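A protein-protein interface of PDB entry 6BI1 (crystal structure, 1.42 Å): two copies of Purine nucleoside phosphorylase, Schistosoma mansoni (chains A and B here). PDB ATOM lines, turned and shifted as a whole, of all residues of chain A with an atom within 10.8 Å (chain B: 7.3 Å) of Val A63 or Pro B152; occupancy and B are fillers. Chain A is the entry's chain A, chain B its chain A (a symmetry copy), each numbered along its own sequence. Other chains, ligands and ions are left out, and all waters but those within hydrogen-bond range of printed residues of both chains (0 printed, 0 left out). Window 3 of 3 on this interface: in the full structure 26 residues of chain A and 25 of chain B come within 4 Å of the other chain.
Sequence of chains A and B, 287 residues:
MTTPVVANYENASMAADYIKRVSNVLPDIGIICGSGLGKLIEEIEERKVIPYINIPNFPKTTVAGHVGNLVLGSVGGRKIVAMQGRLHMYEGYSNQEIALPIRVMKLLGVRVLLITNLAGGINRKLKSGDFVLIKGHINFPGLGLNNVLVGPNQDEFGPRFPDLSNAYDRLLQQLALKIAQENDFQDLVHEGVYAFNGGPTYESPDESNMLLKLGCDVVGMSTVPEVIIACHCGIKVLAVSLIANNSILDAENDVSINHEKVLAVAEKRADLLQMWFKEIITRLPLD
The backbone carbonyl oxygen (O) of Tyr A90 sits at hydrogen-bond distance from the backbone NH (N) of Gly B151, 3.0 Å away.
The backbone nitrogen of Pro B152 lies close to the backbone carbonyl oxygen of Glu A91 (3.5 Å).
Hydrophobic or aromatic side chains of chain B that line the printed part of chain A: Leu B149, Val B150 and Pro B152.
Along chain B the printed residues that touch a printed residue of chain A span positions 149 to 160.
Hydrophobic or aromatic side chains of chain A within 4 Å of the printed part of chain B: Val A63 and Pro A200.
Along chain A the printed residues that touch a printed residue of chain B span positions 63 to 200.
Of the printed residues of chain B, Val A63 touches Pro B152 (3.8 Å).
Of chain A, only Val A63 and Glu A91 come within 4 Å of Pro B152.
Asn B153 touches none of the printed residues of chain A.
No residue of chain A comes within 4 Å of Gln B154.
Printed residues of chain A within 4 Å of Arg B160: Pro A200 (3.4 Å).
Printed residues of chain B within 4 Å of Glu A91: Gly B151 (3.3 Å) and Pro B152 (3.5 Å).
Printed residues of chain B within 4 Å of Gly A199: Val B150.
The nearest printed residue of chain A that does not touch Pro B152 is Tyr A90 (5.2 Å).
The nearest printed residue of chain A that does not touch Leu B149 is Tyr A90 (4.2 Å).
Among the printed residues, merely in contact across the chains: Val A63 with Pro B152 (3.8 Å), Met A89 with Val B150 (3.9 Å), Tyr A90 with Val B150 (3.5 Å), Glu A91 with Gly B151 (3.3 Å), Gly A92 with Gly B151 (3.99 Å), Gly A199 with Val B150 (3.6 Å), Pro A200 with Leu B149 (3.6 Å) and Pro A200 with Arg B160 (3.4 Å).
A ring nitrogen (ND1) of His A88 sits at hydrogen-bond distance from the side-chain hydroxyl (OH) of Tyr A90, 3.1 Å away.
O of Leu B149 sits at hydrogen-bond distance from NH1 of Arg B160 (3.3 Å).
The guanidinium group (NH2) of Arg B160 is in hydrogen-bond range of the backbone carbonyl oxygen (O) of Gly B151 (2.9 Å).
No position is printed for both chains.
Of the 10 pairs that touch across the chains among the printed residues, none has its exchanged pair printed and touching as well.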
ATOM      1  N   ILE A  53     -11.628  -9.972 -23.475  1.00  0.00           N
ATOM      2  CA  ILE A  53     -11.946  -8.551 -23.535  1.00  0.00           C
ATOM      3  C   ILE A  53     -10.952  -7.768 -24.395  1.00  0.00           C
ATOM      4  O   ILE A  53     -11.283  -6.674 -24.864  1.00  0.00           O
ATOM      5  CB  ILE A  53     -12.055  -7.990 -22.092  1.00  0.00           C
ATOM      6  CG1 ILE A  53     -12.641  -6.577 -22.076  1.00  0.00           C
ATOM      7  CG2 ILE A  53     -10.702  -7.971 -21.419  1.00  0.00           C
ATOM      8  CD1 ILE A  53     -13.077  -6.122 -20.679  1.00  0.00           C
ATOM      9  N   PRO A  59     -17.119 -11.855 -27.870  1.00  0.00           N
ATOM     10  CA  PRO A  59     -18.337 -11.495 -27.127  1.00  0.00           C
ATOM     11  C   PRO A  59     -18.031 -10.943 -25.743  1.00  0.00           C
ATOM     12  O   PRO A  59     -17.058 -11.333 -25.092  1.00  0.00           O
ATOM     13  CB  PRO A  59     -19.125 -12.812 -27.047  1.00  0.00           C
ATOM     14  CG  PRO A  59     -18.192 -13.888 -27.449  1.00  0.00           C
ATOM     15  CD  PRO A  59     -17.061 -13.281 -28.227  1.00  0.00           C
ATOM     16  N   LYS A  60     -18.863 -10.003 -25.326  1.00  0.00           N
ATOM     17  CA  LYS A  60     -18.769  -9.408 -23.996  1.00  0.00           C
ATOM     18  C   LYS A  60     -19.294 -10.407 -22.972  1.00  0.00           C
ATOM     19  O   LYS A  60     -20.392 -10.950 -23.133  1.00  0.00           O
ATOM     20  CB  LYS A  60     -19.589  -8.125 -23.938  1.00  0.00           C
ATOM     21  CG  LYS A  60     -19.598  -7.476 -22.556  1.00  0.00           C
ATOM     22  CD  LYS A  60     -20.145  -6.060 -22.590  1.00  0.00           C
ATOM     23  CE  LYS A  60     -20.020  -5.403 -21.221  1.00  0.00           C
ATOM     24  NZ  LYS A  60     -20.674  -4.068 -21.170  1.00  0.00           N
ATOM     25  N   THR A  61     -18.502 -10.662 -21.925  1.00  0.00           N
ATOM     26  CA  THR A  61     -18.847 -11.671 -20.923  1.00  0.00           C
ATOM     27  C   THR A  61     -18.878 -11.109 -19.501  1.00  0.00           C
ATOM     28  O   THR A  61     -18.834 -11.884 -18.539  1.00  0.00           O
ATOM     29  CB  THR A  61     -17.889 -12.869 -20.998  1.00  0.00           C
ATOM     30  OG1 THR A  61     -16.570 -12.480 -20.591  1.00  0.00           O
ATOM     31  CG2 THR A  61     -17.820 -13.419 -22.400  1.00  0.00           C
ATOM     32  N   THR A  62     -18.998  -9.792 -19.328  1.00  0.00           N
ATOM     33  CA  THR A  62     -18.869  -9.243 -17.979  1.00  0.00           C
ATOM     34  C   THR A  62     -20.128  -9.397 -17.137  1.00  0.00           C
ATOM     35  O   THR A  62     -20.031  -9.358 -15.905  1.00  0.00           O
ATOM     36  CB  THR A  62     -18.462  -7.773 -18.018  1.00  0.00           C
ATOM     37  OG1 THR A  62     -19.517  -7.004 -18.599  1.00  0.00           O
ATOM     38  CG2 THR A  62     -17.198  -7.597 -18.831  1.00  0.00           C
ATOM     39  N   VAL A  63     -21.306  -9.552 -17.747  1.00  0.00           N
ATOM     40  CA  VAL A  63     -22.515  -9.749 -16.944  1.00  0.00           C
ATOM     41  C   VAL A  63     -22.428 -11.060 -16.161  1.00  0.00           C
ATOM     42  O   VAL A  63     -22.750 -11.112 -14.967  1.00  0.00           O
ATOM     43  CB  VAL A  63     -23.778  -9.677 -17.824  1.00  0.00           C
ATOM     44  CG1 VAL A  63     -25.012 -10.050 -17.026  1.00  0.00           C
ATOM     45  CG2 VAL A  63     -23.940  -8.279 -18.432  1.00  0.00           C
ATOM     46  N   ALA A  64     -22.014 -12.143 -16.829  1.00  0.00           N
ATOM     47  CA  ALA A  64     -21.819 -13.414 -16.128  1.00  0.00           C
ATOM     48  C   ALA A  64     -20.549 -13.400 -15.284  1.00  0.00           C
ATOM     49  O   ALA A  64     -20.488 -14.072 -14.248  1.00  0.00           O
ATOM     50  CB  ALA A  64     -21.743 -14.576 -17.124  1.00  0.00           C
ATOM     51  N   GLY A  65     -19.519 -12.674 -15.726  1.00  0.00           N
ATOM     52  CA  GLY A  65     -18.294 -12.574 -14.959  1.00  0.00           C
ATOM     53  C   GLY A  65     -17.432 -13.822 -15.066  1.00  0.00           C
ATOM     54  O   GLY A  65     -17.513 -14.607 -16.020  1.00  0.00           O
ATOM     55  N   HIS A  66     -16.604 -14.013 -14.031  1.00  0.00           N
ATOM     56  CA  HIS A  66     -15.694 -15.150 -13.957  1.00  0.00           C
ATOM     57  C   HIS A  66     -14.716 -15.140 -15.132  1.00  0.00           C
ATOM     58  O   HIS A  66     -14.659 -14.165 -15.891  1.00  0.00           O
ATOM     59  CB  HIS A  66     -16.481 -16.465 -13.859  1.00  0.00           C
ATOM     60  CG  HIS A  66     -17.326 -16.569 -12.627  1.00  0.00           C
ATOM     61  ND1 HIS A  66     -18.638 -16.144 -12.578  1.00  0.00           N
ATOM     62  CD2 HIS A  66     -17.039 -17.038 -11.390  1.00  0.00           C
ATOM     63  CE1 HIS A  66     -19.122 -16.349 -11.364  1.00  0.00           C
ATOM     64  NE2 HIS A  66     -18.171 -16.886 -10.621  1.00  0.00           N
ATOM     65  N   VAL A  67     -13.951 -16.222 -15.310  1.00  0.00           N
ATOM     66  CA  VAL A  67     -12.813 -16.191 -16.223  1.00  0.00           C
ATOM     67  C   VAL A  67     -13.270 -16.231 -17.683  1.00  0.00           C
ATOM     68  O   VAL A  67     -14.304 -16.823 -18.028  1.00  0.00           O
ATOM     69  CB  VAL A  67     -11.842 -17.347 -15.909  1.00  0.00           C
ATOM     70  CG1 VAL A  67     -12.460 -18.689 -16.273  1.00  0.00           C
ATOM     71  CG2 VAL A  67     -10.501 -17.149 -16.626  1.00  0.00           C
ATOM     72  N   GLY A  68     -12.473 -15.602 -18.558  1.00  0.00           N
ATOM     73  CA  GLY A  68     -12.677 -15.661 -19.998  1.00  0.00           C
ATOM     74  C   GLY A  68     -11.407 -15.335 -20.776  1.00  0.00           C
ATOM     75  O   GLY A  68     -11.127 -14.159 -21.059  1.00  0.00           O
ATOM     76  N   LEU A  87     -18.765 -20.332 -23.187  1.00  0.00           N
ATOM     77  CA  LEU A  87     -19.992 -19.593 -23.452  1.00  0.00           C
ATOM     78  C   LEU A  87     -21.121 -20.603 -23.634  1.00  0.00           C
ATOM     79  O   LEU A  87     -21.034 -21.456 -24.526  1.00  0.00           O
ATOM     80  CB  LEU A  87     -19.826 -18.816 -24.762  1.00  0.00           C
ATOM     81  CG  LEU A  87     -18.610 -17.913 -24.884  1.00  0.00           C
ATOM     82  CD1 LEU A  87     -18.405 -17.558 -26.354  1.00  0.00           C
ATOM     83  CD2 LEU A  87     -18.808 -16.679 -24.050  1.00  0.00           C
ATOM     84  N   HIS A  88     -22.165 -20.518 -22.799  1.00  0.00           N
ATOM     85  CA  HIS A  88     -23.339 -21.393 -22.867  1.00  0.00           C
ATOM     86  C   HIS A  88     -24.604 -20.630 -23.285  1.00  0.00           C
ATOM     87  O   HIS A  88     -24.852 -19.496 -22.844  1.00  0.00           O
ATOM     88  CB  HIS A  88     -23.609 -22.055 -21.506  1.00  0.00           C
ATOM     89  CG  HIS A  88     -22.542 -22.996 -21.027  1.00  0.00           C
ATOM     90  ND1 HIS A  88     -21.649 -22.661 -20.029  1.00  0.00           N
ATOM     91  CD2 HIS A  88     -22.255 -24.271 -21.373  1.00  0.00           C
ATOM     92  CE1 HIS A  88     -20.857 -23.690 -19.784  1.00  0.00           C
ATOM     93  NE2 HIS A  88     -21.201 -24.678 -20.588  1.00  0.00           N
ATOM     94  N   MET A  89     -25.461 -21.282 -24.086  1.00  0.00           N
ATOM     95  CA  MET A  89     -26.641 -20.579 -24.609  1.00  0.00           C
ATOM     96  C   MET A  89     -27.679 -20.278 -23.526  1.00  0.00           C
ATOM     97  O   MET A  89     -28.418 -19.289 -23.657  1.00  0.00           O
ATOM     98  CB  MET A  89     -27.193 -21.316 -25.832  1.00  0.00           C
ATOM     99  CG  MET A  89     -26.115 -21.432 -26.950  1.00  0.00           C
ATOM    100  SD  MET A  89     -26.679 -21.652 -28.668  1.00  0.00           S
ATOM    101  CE  MET A  89     -27.531 -20.092 -28.917  1.00  0.00           C
ATOM    102  N   TYR A  90     -27.741 -21.069 -22.435  1.00  0.00           N
ATOM    103  CA  TYR A  90     -28.674 -20.735 -21.349  1.00  0.00           C
ATOM    104  C   TYR A  90     -28.338 -19.411 -20.664  1.00  0.00           C
ATOM    105  O   TYR A  90     -29.170 -18.890 -19.898  1.00  0.00           O
ATOM    106  CB  TYR A  90     -28.774 -21.851 -20.296  1.00  0.00           C
ATOM    107  CG  TYR A  90     -27.474 -22.234 -19.662  1.00  0.00           C
ATOM    108  CD1 TYR A  90     -26.861 -21.404 -18.714  1.00  0.00           C
ATOM    109  CD2 TYR A  90     -26.861 -23.425 -19.990  1.00  0.00           C
ATOM    110  CE1 TYR A  90     -25.644 -21.754 -18.149  1.00  0.00           C
ATOM    111  CE2 TYR A  90     -25.644 -23.789 -19.428  1.00  0.00           C
ATOM    112  CZ  TYR A  90     -25.031 -22.955 -18.512  1.00  0.00           C
ATOM    113  OH  TYR A  90     -23.817 -23.341 -17.937  1.00  0.00           O
ATOM    114  N   GLU A  91     -27.133 -18.851 -20.876  1.00  0.00           N
ATOM    115  CA  GLU A  91     -26.761 -17.568 -20.297  1.00  0.00           C
ATOM    116  C   GLU A  91     -27.332 -16.396 -21.084  1.00  0.00           C
ATOM    117  O   GLU A  91     -27.280 -15.252 -20.590  1.00  0.00           O
ATOM    118  CB  GLU A  91     -25.225 -17.484 -20.182  1.00  0.00           C
ATOM    119  N   GLY A  92     -27.897 -16.649 -22.264  1.00  0.00           N
ATOM    120  CA  GLY A  92     -28.447 -15.615 -23.119  1.00  0.00           C
ATOM    121  C   GLY A  92     -27.573 -15.179 -24.282  1.00  0.00           C
ATOM    122  O   GLY A  92     -27.983 -14.270 -25.007  1.00  0.00           O
ATOM    123  N   TYR A  93     -26.387 -15.762 -24.458  1.00  0.00           N
ATOM    124  CA  TYR A  93     -25.559 -15.444 -25.626  1.00  0.00           C
ATOM    125  C   TYR A  93     -26.297 -15.808 -26.917  1.00  0.00           C
ATOM    126  O   TYR A  93     -27.006 -16.818 -26.986  1.00  0.00           O
ATOM    127  CB  TYR A  93     -24.217 -16.202 -25.558  1.00  0.00           C
ATOM    128  CG  TYR A  93     -23.344 -15.798 -24.373  1.00  0.00           C
ATOM    129  CD1 TYR A  93     -22.780 -14.538 -24.307  1.00  0.00           C
ATOM    130  CD2 TYR A  93     -23.071 -16.681 -23.330  1.00  0.00           C
ATOM    131  CE1 TYR A  93     -21.991 -14.152 -23.219  1.00  0.00           C
ATOM    132  CE2 TYR A  93     -22.310 -16.316 -22.263  1.00  0.00           C
ATOM    133  CZ  TYR A  93     -21.769 -15.043 -22.196  1.00  0.00           C
ATOM    134  OH  TYR A  93     -20.987 -14.658 -21.127  1.00  0.00           O
ATOM    135  N   SER A  94     -26.108 -14.997 -27.962  1.00  0.00           N
ATOM    136  CA  SER A  94     -26.735 -15.269 -29.257  1.00  0.00           C
ATOM    137  C   SER A  94     -25.954 -16.300 -30.070  1.00  0.00           C
ATOM    138  O   SER A  94     -24.804 -16.630 -29.772  1.00  0.00           O
ATOM    139  CB  SER A  94     -26.805 -13.993 -30.085  1.00  0.00           C
ATOM    140  OG  SER A  94     -25.528 -13.642 -30.569  1.00  0.00           O
ATOM    141  N   GLU A  97     -22.604 -14.938 -31.109  1.00  0.00           N
ATOM    142  CA  GLU A  97     -21.581 -14.908 -30.058  1.00  0.00           C
ATOM    143  C   GLU A  97     -20.953 -16.290 -29.834  1.00  0.00           C
ATOM    144  O   GLU A  97     -19.738 -16.396 -29.631  1.00  0.00           O
ATOM    145  CB  GLU A  97     -22.184 -14.337 -28.772  1.00  0.00           C
ATOM    146  CG  GLU A  97     -22.535 -12.846 -28.835  1.00  0.00           C
ATOM    147  CD  GLU A  97     -23.247 -12.315 -27.596  1.00  0.00           C
ATOM    148  OE1 GLU A  97     -24.342 -12.803 -27.239  1.00  0.00           O
ATOM    149  OE2 GLU A  97     -22.714 -11.348 -26.988  1.00  0.00           O
ATOM    150  N   GLY A 199     -31.725 -25.755 -21.175  1.00  0.00           N
ATOM    151  CA  GLY A 199     -31.447 -25.355 -19.791  1.00  0.00           C
ATOM    152  C   GLY A 199     -31.980 -23.971 -19.406  1.00  0.00           C
ATOM    153  O   GLY A 199     -32.691 -23.327 -20.209  1.00  0.00           O
ATOM    154  N   PRO A 200     -31.639 -23.474 -18.202  1.00  0.00           N
ATOM    155  CA  PRO A 200     -30.645 -23.972 -17.229  1.00  0.00           C
ATOM    156  C   PRO A 200     -31.209 -24.874 -16.136  1.00  0.00           C
ATOM    157  O   PRO A 200     -30.434 -25.302 -15.271  1.00  0.00           O
ATOM    158  CB  PRO A 200     -30.132 -22.663 -16.595  1.00  0.00           C
ATOM    159  CG  PRO A 200     -31.373 -21.779 -16.563  1.00  0.00           C
ATOM    160  CD  PRO A 200     -32.081 -22.104 -17.863  1.00  0.00           C
ATOM    161  N   VAL B   6     -35.465  -5.678 -16.557  1.00  0.00           N
ATOM    162  CA  VAL B   6     -35.011  -6.985 -16.082  1.00  0.00           C
ATOM    163  C   VAL B   6     -35.694  -7.328 -14.765  1.00  0.00           C
ATOM    164  O   VAL B   6     -35.912  -6.450 -13.913  1.00  0.00           O
ATOM    165  CB  VAL B   6     -33.479  -6.998 -15.933  1.00  0.00           C
ATOM    166  CG1 VAL B   6     -32.957  -8.316 -15.334  1.00  0.00           C
ATOM    167  CG2 VAL B   6     -32.830  -6.743 -17.298  1.00  0.00           C
ATOM    168  N   GLN B  96     -38.420 -11.974 -18.788  1.00  0.00           N
ATOM    169  CA  GLN B  96     -38.324 -11.011 -17.697  1.00  0.00           C
ATOM    170  C   GLN B  96     -39.696 -10.494 -17.272  1.00  0.00           C
ATOM    171  O   GLN B  96     -39.919 -10.228 -16.083  1.00  0.00           O
ATOM    172  CB  GLN B  96     -37.438  -9.831 -18.105  1.00  0.00           C
ATOM    173  CG  GLN B  96     -36.030 -10.177 -18.620  1.00  0.00           C
ATOM    174  CD  GLN B  96     -35.121 -10.740 -17.534  1.00  0.00           C
ATOM    175  OE1 GLN B  96     -35.409 -10.713 -16.337  1.00  0.00           O
ATOM    176  NE2 GLN B  96     -33.965 -11.231 -17.974  1.00  0.00           N
ATOM    177  N   ARG B 103     -41.571 -12.785  -8.600  1.00  0.00           N
ATOM    178  CA  ARG B 103     -40.496 -12.351  -7.703  1.00  0.00           C
ATOM    179  C   ARG B 103     -40.943 -11.231  -6.764  1.00  0.00           C
ATOM    180  O   ARG B 103     -40.469 -11.145  -5.611  1.00  0.00           O
ATOM    181  CB  ARG B 103     -39.274 -11.976  -8.556  1.00  0.00           C
ATOM    182  CG  ARG B 103     -38.599 -13.220  -9.152  1.00  0.00           C
ATOM    183  CD  ARG B 103     -37.396 -12.966 -10.082  1.00  0.00           C
ATOM    184  NE  ARG B 103     -36.751 -14.231 -10.451  1.00  0.00           N
ATOM    185  CZ  ARG B 103     -35.851 -14.374 -11.404  1.00  0.00           C
ATOM    186  NH1 ARG B 103     -35.467 -13.341 -12.162  1.00  0.00           N
ATOM    187  NH2 ARG B 103     -35.365 -15.582 -11.674  1.00  0.00           N
ATOM    188  N   LEU B 149     -35.958 -19.229 -17.579  1.00  0.00           N
ATOM    189  CA  LEU B 149     -34.729 -18.802 -16.904  1.00  0.00           C
ATOM    190  C   LEU B 149     -33.546 -18.541 -17.861  1.00  0.00           C
ATOM    191  O   LEU B 149     -32.448 -18.221 -17.381  1.00  0.00           O
ATOM    192  CB  LEU B 149     -34.342 -19.822 -15.794  1.00  0.00           C
ATOM    193  CG  LEU B 149     -35.201 -19.830 -14.521  1.00  0.00           C
ATOM    194  CD1 LEU B 149     -34.829 -21.008 -13.635  1.00  0.00           C
ATOM    195  CD2 LEU B 149     -35.014 -18.523 -13.734  1.00  0.00           C
ATOM    196  N   VAL B 150     -33.701 -18.690 -19.198  1.00  0.00           N
ATOM    197  CA  VAL B 150     -32.602 -18.319 -20.110  1.00  0.00           C
ATOM    198  C   VAL B 150     -32.280 -16.837 -19.932  1.00  0.00           C
ATOM    199  O   VAL B 150     -33.168 -15.964 -20.034  1.00  0.00           O
ATOM    200  CB  VAL B 150     -32.958 -18.647 -21.572  1.00  0.00           C
ATOM    201  CG1 VAL B 150     -31.956 -18.043 -22.541  1.00  0.00           C
ATOM    202  CG2 VAL B 150     -33.042 -20.146 -21.791  1.00  0.00           C
ATOM    203  N   GLY B 151     -30.986 -16.539 -19.744  1.00  0.00           N
ATOM    204  CA  GLY B 151     -30.511 -15.199 -19.422  1.00  0.00           C
ATOM    205  C   GLY B 151     -29.565 -15.234 -18.227  1.00  0.00           C
ATOM    206  O   GLY B 151     -29.286 -16.311 -17.671  1.00  0.00           O
ATOM    207  N   PRO B 152     -29.019 -14.084 -17.826  1.00  0.00           N
ATOM    208  CA  PRO B 152     -28.230 -14.025 -16.585  1.00  0.00           C
ATOM    209  C   PRO B 152     -29.046 -14.561 -15.415  1.00  0.00           C
ATOM    210  O   PRO B 152     -30.249 -14.342 -15.326  1.00  0.00           O
ATOM    211  CB  PRO B 152     -27.952 -12.523 -16.403  1.00  0.00           C
ATOM    212  CG  PRO B 152     -28.315 -11.857 -17.693  1.00  0.00           C
ATOM    213  CD  PRO B 152     -29.244 -12.771 -18.453  1.00  0.00           C
ATOM    214  N   ASN B 153     -28.385 -15.235 -14.481  1.00  0.00           N
ATOM    215  CA  ASN B 153     -29.068 -15.628 -13.249  1.00  0.00           C
ATOM    216  C   ASN B 153     -29.167 -14.442 -12.281  1.00  0.00           C
ATOM    217  O   ASN B 153     -28.204 -13.685 -12.102  1.00  0.00           O
ATOM    218  CB  ASN B 153     -28.371 -16.801 -12.550  1.00  0.00           C
ATOM    219  CG  ASN B 153     -29.212 -17.345 -11.390  1.00  0.00           C
ATOM    220  OD1 ASN B 153     -30.363 -17.762 -11.593  1.00  0.00           O
ATOM    221  ND2 ASN B 153     -28.656 -17.331 -10.188  1.00  0.00           N
ATOM    222  N   GLN B 154     -30.339 -14.297 -11.646  1.00  0.00           N
ATOM    223  CA  GLN B 154     -30.538 -13.309 -10.574  1.00  0.00           C
ATOM    224  C   GLN B 154     -30.288 -14.031  -9.244  1.00  0.00           C
ATOM    225  O   GLN B 154     -31.180 -14.683  -8.675  1.00  0.00           O
ATOM    226  CB  GLN B 154     -31.920 -12.665 -10.680  1.00  0.00           C
ATOM    227  CG  GLN B 154     -32.193 -12.012 -12.048  1.00  0.00           C
ATOM    228  CD  GLN B 154     -31.176 -10.929 -12.456  1.00  0.00           C
ATOM    229  OE1 GLN B 154     -30.591 -10.258 -11.602  1.00  0.00           O
ATOM    230  NE2 GLN B 154     -30.983 -10.745 -13.759  1.00  0.00           N
ATOM    231  N   ASP B 155     -29.036 -13.935  -8.771  1.00  0.00           N
ATOM    232  CA  ASP B 155     -28.557 -14.750  -7.651  1.00  0.00           C
ATOM    233  C   ASP B 155     -29.313 -14.495  -6.336  1.00  0.00           C
ATOM    234  O   ASP B 155     -29.424 -15.407  -5.499  1.00  0.00           O
ATOM    235  CB  ASP B 155     -27.058 -14.504  -7.436  1.00  0.00           C
ATOM    236  CG  ASP B 155     -26.204 -14.931  -8.629  1.00  0.00           C
ATOM    237  OD1 ASP B 155     -26.344 -16.070  -9.132  1.00  0.00           O
ATOM    238  OD2 ASP B 155     -25.325 -14.136  -9.037  1.00  0.00           O
ATOM    239  N   ARG B 160     -28.190 -20.895 -10.159  1.00  0.00           N
ATOM    240  CA  ARG B 160     -28.029 -20.940 -11.618  1.00  0.00           C
ATOM    241  C   ARG B 160     -28.720 -22.150 -12.240  1.00  0.00           C
ATOM    242  O   ARG B 160     -29.359 -22.018 -13.307  1.00  0.00           O
ATOM    243  CB  ARG B 160     -26.530 -20.901 -11.979  1.00  0.00           C
ATOM    244  CG  ARG B 160     -26.188 -21.140 -13.473  1.00  0.00           C
ATOM    245  CD  ARG B 160     -26.465 -20.006 -14.430  1.00  0.00           C
ATOM    246  NE  ARG B 160     -27.879 -19.796 -14.735  1.00  0.00           N
ATOM    247  CZ  ARG B 160     -28.327 -18.905 -15.617  1.00  0.00           C
ATOM    248  NH1 ARG B 160     -29.627 -18.727 -15.797  1.00  0.00           N
ATOM    249  NH2 ARG B 160     -27.457 -18.157 -16.303  1.00  0.00           N
